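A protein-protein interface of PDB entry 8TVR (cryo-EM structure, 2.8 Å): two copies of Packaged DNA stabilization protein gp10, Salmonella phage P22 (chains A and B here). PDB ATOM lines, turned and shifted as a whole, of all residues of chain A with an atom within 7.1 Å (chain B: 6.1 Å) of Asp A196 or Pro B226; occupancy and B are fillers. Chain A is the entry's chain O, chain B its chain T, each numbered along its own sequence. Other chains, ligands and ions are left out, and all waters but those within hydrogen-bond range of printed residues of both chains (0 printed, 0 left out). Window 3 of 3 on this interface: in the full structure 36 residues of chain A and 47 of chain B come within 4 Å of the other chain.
NH1 of Arg A148 touches N of Ser B183, at 3.6 Å.
OD2 of Asp A196 touches CB of Pro B226, 3.9 Å away.
Of the 8 printed residues of chain B, 4 touch a printed residue of chain A.
Hydrophobic or aromatic side chains of chain B within 4 Å of the printed part of chain A: Pro B226 and Met B229.
Of the 12 printed residues of chain A, 3 touch a printed residue of chain B.
Among the printed residues, 6 pairs touch across the chains.
Among the printed residues, no Asp or Glu carboxylate lies within 4 Å of a Lys or Arg side-chain nitrogen of the other chain.
No position is printed for both chains.
The guanidinium group of Arg A195 is in hydrogen-bond range of the backbone carbonyl oxygen of Ser B227 (2.8 Å).
NH1 of Arg A195 lies within hydrogen-bond range of O of Met B229.
The guanidinium group (NH2) of Arg A195 sits at hydrogen-bond distance from the backbone carbonyl oxygen (O) of Pro B226 (3.3 Å).
OD1 of Asp A196 lies within hydrogen-bond range of OG of Ser B183 (3.1 Å).
The guanidinium group (NH2) of Arg A148 lies within salt-bridge range of the side-chain carboxylate (OD2) of Asp A196.
Asp A196 touches just these residues of chain B: Ser B183 and Pro B226.
Pro B226 touches just these residues of chain A: Arg A195 and Asp A196.
Of the printed residues of chain B, Arg A195 touches Pro B226, Ser B227 and Met B229.
Of the printed residues of chain A, Ser B183 touches Arg A148 and Asp A196.
Gln B225 touches none of the printed residues of chain A.
The nearest residue of chain B that does not touch Asp A196 is Met B229 (5.2 Å).
The nearest residue of chain A that does not touch Pro B226 is Arg A148 (5.0 Å).
The nearest printed residue of chain B that does not touch Arg A148 is Ala B224 (4.5 Å).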
ATOM      1  N   LEU A 147      13.347  -3.416  -0.106  1.00  0.00           N
ATOM      2  CA  LEU A 147      12.395  -2.330   0.085  1.00  0.00           C
ATOM      3  C   LEU A 147      13.153  -1.038   0.342  1.00  0.00           C
ATOM      4  O   LEU A 147      14.076  -1.015   1.163  1.00  0.00           O
ATOM      5  CB  LEU A 147      11.439  -2.620   1.247  1.00  0.00           C
ATOM      6  CG  LEU A 147      10.406  -1.530   1.548  1.00  0.00           C
ATOM      7  CD1 LEU A 147       9.267  -1.567   0.542  1.00  0.00           C
ATOM      8  CD2 LEU A 147       9.873  -1.651   2.963  1.00  0.00           C
ATOM      9  N   ARG A 148      12.760   0.025  -0.363  1.00  0.00           N
ATOM     10  CA  ARG A 148      13.278   1.376  -0.133  1.00  0.00           C
ATOM     11  C   ARG A 148      14.804   1.411  -0.169  1.00  0.00           C
ATOM     12  O   ARG A 148      15.451   2.088   0.633  1.00  0.00           O
ATOM     13  CB  ARG A 148      12.752   1.944   1.185  1.00  0.00           C
ATOM     14  CG  ARG A 148      11.273   2.283   1.171  1.00  0.00           C
ATOM     15  CD  ARG A 148      11.015   3.576   0.420  1.00  0.00           C
ATOM     16  NE  ARG A 148       9.620   3.991   0.505  1.00  0.00           N
ATOM     17  CZ  ARG A 148       9.123   5.072  -0.080  1.00  0.00           C
ATOM     18  NH1 ARG A 148       9.883   5.878  -0.803  1.00  0.00           N
ATOM     19  NH2 ARG A 148       7.831   5.352   0.066  1.00  0.00           N
ATOM     20  N   THR A 193       7.592  -8.133   1.006  1.00  0.00           N
ATOM     21  CA  THR A 193       7.194  -6.729   1.029  1.00  0.00           C
ATOM     22  C   THR A 193       5.850  -6.603   0.332  1.00  0.00           C
ATOM     23  O   THR A 193       5.741  -6.900  -0.861  1.00  0.00           O
ATOM     24  CB  THR A 193       8.238  -5.840   0.348  1.00  0.00           C
ATOM     25  OG1 THR A 193       8.639  -6.436  -0.891  1.00  0.00           O
ATOM     26  CG2 THR A 193       9.457  -5.675   1.236  1.00  0.00           C
ATOM     27  N   TRP A 194       4.826  -6.177   1.072  1.00  0.00           N
ATOM     28  CA  TRP A 194       3.471  -6.122   0.513  1.00  0.00           C
ATOM     29  C   TRP A 194       3.230  -4.839  -0.278  1.00  0.00           C
ATOM     30  O   TRP A 194       3.122  -4.871  -1.507  1.00  0.00           O
ATOM     31  CB  TRP A 194       2.445  -6.278   1.638  1.00  0.00           C
ATOM     32  CG  TRP A 194       1.048  -5.975   1.222  1.00  0.00           C
ATOM     33  CD1 TRP A 194       0.415  -6.408   0.097  1.00  0.00           C
ATOM     34  CD2 TRP A 194       0.102  -5.169   1.931  1.00  0.00           C
ATOM     35  NE1 TRP A 194      -0.867  -5.920   0.059  1.00  0.00           N
ATOM     36  CE2 TRP A 194      -1.084  -5.157   1.175  1.00  0.00           C
ATOM     37  CE3 TRP A 194       0.144  -4.456   3.132  1.00  0.00           C
ATOM     38  CZ2 TRP A 194      -2.218  -4.460   1.581  1.00  0.00           C
ATOM     39  CZ3 TRP A 194      -0.980  -3.765   3.532  1.00  0.00           C
ATOM     40  CH2 TRP A 194      -2.146  -3.772   2.760  1.00  0.00           C
ATOM     41  N   ARG A 195       3.163  -3.699   0.410  1.00  0.00           N
ATOM     42  CA  ARG A 195       3.033  -2.412  -0.265  1.00  0.00           C
ATOM     43  C   ARG A 195       4.195  -1.485   0.056  1.00  0.00           C
ATOM     44  O   ARG A 195       4.925  -1.070  -0.850  1.00  0.00           O
ATOM     45  CB  ARG A 195       1.699  -1.756   0.115  1.00  0.00           C
ATOM     46  CG  ARG A 195       0.614  -1.937  -0.925  1.00  0.00           C
ATOM     47  CD  ARG A 195      -0.772  -1.755  -0.331  1.00  0.00           C
ATOM     48  NE  ARG A 195      -1.141  -0.350  -0.200  1.00  0.00           N
ATOM     49  CZ  ARG A 195      -1.488   0.436  -1.210  1.00  0.00           C
ATOM     50  NH1 ARG A 195      -1.518  -0.007  -2.455  1.00  0.00           N
ATOM     51  NH2 ARG A 195      -1.818   1.700  -0.964  1.00  0.00           N
ATOM     52  N   ASP A 196       4.390  -1.159   1.332  1.00  0.00           N
ATOM     53  CA  ASP A 196       5.566  -0.440   1.801  1.00  0.00           C
ATOM     54  C   ASP A 196       5.999  -0.987   3.154  1.00  0.00           C
ATOM     55  O   ASP A 196       6.730  -0.312   3.888  1.00  0.00           O
ATOM     56  CB  ASP A 196       5.298   1.065   1.891  1.00  0.00           C
ATOM     57  CG  ASP A 196       6.443   1.895   1.342  1.00  0.00           C
ATOM     58  OD1 ASP A 196       7.156   1.406   0.441  1.00  0.00           O
ATOM     59  OD2 ASP A 196       6.629   3.038   1.807  1.00  0.00           O
ATOM     60  N   PHE A 197       5.551  -2.190   3.495  1.00  0.00           N
ATOM     61  CA  PHE A 197       5.843  -2.844   4.756  1.00  0.00           C
ATOM     62  C   PHE A 197       6.793  -4.010   4.524  1.00  0.00           C
ATOM     63  O   PHE A 197       6.797  -4.625   3.456  1.00  0.00           O
ATOM     64  CB  PHE A 197       4.564  -3.371   5.420  1.00  0.00           C
ATOM     65  CG  PHE A 197       3.505  -2.329   5.629  1.00  0.00           C
ATOM     66  CD1 PHE A 197       3.452  -1.604   6.807  1.00  0.00           C
ATOM     67  CD2 PHE A 197       2.548  -2.089   4.658  1.00  0.00           C
ATOM     68  CE1 PHE A 197       2.475  -0.650   7.005  1.00  0.00           C
ATOM     69  CE2 PHE A 197       1.568  -1.136   4.851  1.00  0.00           C
ATOM     70  CZ  PHE A 197       1.532  -0.416   6.026  1.00  0.00           C
ATOM     71  N   ILE A 198       7.601  -4.300   5.532  1.00  0.00           N
ATOM     72  CA  ILE A 198       8.301  -5.572   5.616  1.00  0.00           C
ATOM     73  C   ILE A 198       7.375  -6.556   6.310  1.00  0.00           C
ATOM     74  O   ILE A 198       6.930  -6.313   7.436  1.00  0.00           O
ATOM     75  CB  ILE A 198       9.628  -5.428   6.380  1.00  0.00           C
ATOM     76  CG1 ILE A 198      10.500  -4.345   5.745  1.00  0.00           C
ATOM     77  CG2 ILE A 198      10.361  -6.760   6.424  1.00  0.00           C
ATOM     78  CD1 ILE A 198      11.120  -4.751   4.432  1.00  0.00           C
ATOM     79  N   PHE A 209       5.725  -4.394   9.230  1.00  0.00           N
ATOM     80  CA  PHE A 209       6.625  -3.360   9.725  1.00  0.00           C
ATOM     81  C   PHE A 209       6.646  -2.197   8.746  1.00  0.00           C
ATOM     82  O   PHE A 209       6.742  -2.406   7.534  1.00  0.00           O
ATOM     83  CB  PHE A 209       8.047  -3.904   9.915  1.00  0.00           C
ATOM     84  CG  PHE A 209       8.193  -4.837  11.083  1.00  0.00           C
ATOM     85  CD1 PHE A 209       7.747  -6.144  11.005  1.00  0.00           C
ATOM     86  CD2 PHE A 209       8.783  -4.406  12.256  1.00  0.00           C
ATOM     87  CE1 PHE A 209       7.879  -7.002  12.078  1.00  0.00           C
ATOM     88  CE2 PHE A 209       8.921  -5.259  13.332  1.00  0.00           C
ATOM     89  CZ  PHE A 209       8.469  -6.559  13.242  1.00  0.00           C
ATOM     90  N   SER A 210       6.570  -0.978   9.270  1.00  0.00           N
ATOM     91  CA  SER A 210       6.641   0.226   8.458  1.00  0.00           C
ATOM     92  C   SER A 210       7.857   1.052   8.857  1.00  0.00           C
ATOM     93  O   SER A 210       8.444   0.858   9.924  1.00  0.00           O
ATOM     94  CB  SER A 210       5.371   1.074   8.595  1.00  0.00           C
ATOM     95  OG  SER A 210       5.082   1.338   9.955  1.00  0.00           O
ATOM     96  N   LEU A 211       8.229   1.983   7.981  1.00  0.00           N
ATOM     97  CA  LEU A 211       9.363   2.861   8.236  1.00  0.00           C
ATOM     98  C   LEU A 211       8.971   3.943   9.236  1.00  0.00           C
ATOM     99  O   LEU A 211       7.936   4.597   9.082  1.00  0.00           O
ATOM    100  CB  LEU A 211       9.853   3.493   6.935  1.00  0.00           C
ATOM    101  CG  LEU A 211      10.921   2.735   6.142  1.00  0.00           C
ATOM    102  CD1 LEU A 211      11.120   3.366   4.775  1.00  0.00           C
ATOM    103  CD2 LEU A 211      12.234   2.687   6.902  1.00  0.00           C
ATOM    104  N   TYR A 222      12.318   0.792  11.766  1.00  0.00           N
ATOM    105  CA  TYR A 222      11.089   0.081  11.458  1.00  0.00           C
ATOM    106  C   TYR A 222      10.297  -0.142  12.738  1.00  0.00           C
ATOM    107  O   TYR A 222      10.867  -0.332  13.816  1.00  0.00           O
ATOM    108  CB  TYR A 222      11.368  -1.263  10.772  1.00  0.00           C
ATOM    109  CG  TYR A 222      11.650  -1.139   9.293  1.00  0.00           C
ATOM    110  CD1 TYR A 222      10.615  -0.999   8.379  1.00  0.00           C
ATOM    111  CD2 TYR A 222      12.950  -1.155   8.812  1.00  0.00           C
ATOM    112  CE1 TYR A 222      10.866  -0.882   7.027  1.00  0.00           C
ATOM    113  CE2 TYR A 222      13.212  -1.037   7.462  1.00  0.00           C
ATOM    114  CZ  TYR A 222      12.166  -0.901   6.574  1.00  0.00           C
ATOM    115  OH  TYR A 222      12.424  -0.785   5.228  1.00  0.00           O
ATOM    116  N   SER B 183      10.260   3.682  -3.629  1.00  0.00           N
ATOM    117  CA  SER B 183       9.612   2.443  -3.200  1.00  0.00           C
ATOM    118  C   SER B 183       9.607   1.422  -4.328  1.00  0.00           C
ATOM    119  O   SER B 183       8.600   0.781  -4.625  1.00  0.00           O
ATOM    120  CB  SER B 183       8.198   2.731  -2.710  1.00  0.00           C
ATOM    121  OG  SER B 183       7.436   1.539  -2.623  1.00  0.00           O
ATOM    122  N   TYR B 208       2.450   8.436  -5.398  1.00  0.00           N
ATOM    123  CA  TYR B 208       1.779   9.721  -5.263  1.00  0.00           C
ATOM    124  C   TYR B 208       2.583  10.623  -4.337  1.00  0.00           C
ATOM    125  O   TYR B 208       3.073  10.176  -3.296  1.00  0.00           O
ATOM    126  CB  TYR B 208       0.362   9.545  -4.708  1.00  0.00           C
ATOM    127  CG  TYR B 208      -0.635   8.998  -5.704  1.00  0.00           C
ATOM    128  CD1 TYR B 208      -0.590   7.669  -6.104  1.00  0.00           C
ATOM    129  CD2 TYR B 208      -1.627   9.808  -6.236  1.00  0.00           C
ATOM    130  CE1 TYR B 208      -1.500   7.165  -7.009  1.00  0.00           C
ATOM    131  CE2 TYR B 208      -2.541   9.314  -7.143  1.00  0.00           C
ATOM    132  CZ  TYR B 208      -2.473   7.992  -7.527  1.00  0.00           C
ATOM    133  OH  TYR B 208      -3.385   7.499  -8.431  1.00  0.00           O
ATOM    134  N   ALA B 224       5.933  11.573  -0.344  1.00  0.00           N
ATOM    135  CA  ALA B 224       5.185  10.473  -0.932  1.00  0.00           C
ATOM    136  C   ALA B 224       4.043  10.042  -0.022  1.00  0.00           C
ATOM    137  O   ALA B 224       4.170  10.052   1.206  1.00  0.00           O
ATOM    138  CB  ALA B 224       6.107   9.287  -1.211  1.00  0.00           C
ATOM    139  N   GLN B 225       2.923   9.665  -0.634  1.00  0.00           N
ATOM    140  CA  GLN B 225       1.778   9.133   0.092  1.00  0.00           C
ATOM    141  C   GLN B 225       1.692   7.629  -0.132  1.00  0.00           C
ATOM    142  O   GLN B 225       1.108   7.182  -1.126  1.00  0.00           O
ATOM    143  CB  GLN B 225       0.484   9.818  -0.350  1.00  0.00           C
ATOM    144  CG  GLN B 225       0.589  11.328  -0.470  1.00  0.00           C
ATOM    145  CD  GLN B 225       0.694  12.014   0.878  1.00  0.00           C
ATOM    146  OE1 GLN B 225       1.442  12.976   1.042  1.00  0.00           O
ATOM    147  NE2 GLN B 225      -0.057  11.517   1.854  1.00  0.00           N
ATOM    148  N   PRO B 226       2.267   6.820   0.762  1.00  0.00           N
ATOM    149  CA  PRO B 226       2.245   5.364   0.554  1.00  0.00           C
ATOM    150  C   PRO B 226       0.855   4.760   0.595  1.00  0.00           C
ATOM    151  O   PRO B 226       0.663   3.662   0.058  1.00  0.00           O
ATOM    152  CB  PRO B 226       3.117   4.834   1.699  1.00  0.00           C
ATOM    153  CG  PRO B 226       3.030   5.883   2.751  1.00  0.00           C
ATOM    154  CD  PRO B 226       2.922   7.191   2.027  1.00  0.00           C
ATOM    155  N   SER B 227      -0.117   5.431   1.213  1.00  0.00           N
ATOM    156  CA  SER B 227      -1.470   4.895   1.289  1.00  0.00           C
ATOM    157  C   SER B 227      -2.177   4.909  -0.060  1.00  0.00           C
ATOM    158  O   SER B 227      -3.091   4.107  -0.274  1.00  0.00           O
ATOM    159  CB  SER B 227      -2.287   5.682   2.312  1.00  0.00           C
ATOM    160  OG  SER B 227      -3.619   5.205   2.377  1.00  0.00           O
ATOM    161  N   LEU B 228      -1.778   5.797  -0.968  1.00  0.00           N
ATOM    162  CA  LEU B 228      -2.392   5.912  -2.282  1.00  0.00           C
ATOM    163  C   LEU B 228      -1.653   5.124  -3.356  1.00  0.00           C
ATOM    164  O   LEU B 228      -2.045   5.181  -4.525  1.00  0.00           O
ATOM    165  CB  LEU B 228      -2.472   7.385  -2.692  1.00  0.00           C
ATOM    166  CG  LEU B 228      -3.525   8.240  -1.988  1.00  0.00           C
ATOM    167  CD1 LEU B 228      -3.555   9.635  -2.583  1.00  0.00           C
ATOM    168  CD2 LEU B 228      -4.892   7.586  -2.079  1.00  0.00           C
ATOM    169  N   MET B 229      -0.606   4.392  -2.988  1.00  0.00           N
ATOM    170  CA  MET B 229       0.234   3.715  -3.965  1.00  0.00           C
ATOM    171  C   MET B 229      -0.523   2.585  -4.656  1.00  0.00           C
ATOM    172  O   MET B 229      -1.398   1.942  -4.072  1.00  0.00           O
ATOM    173  CB  MET B 229       1.489   3.165  -3.288  1.00  0.00           C
ATOM    174  CG  MET B 229       2.665   2.946  -4.222  1.00  0.00           C
ATOM    175  SD  MET B 229       3.727   1.590  -3.691  1.00  0.00           S
ATOM    176  CE  MET B 229       2.507   0.349  -3.269  1.00  0.00           C
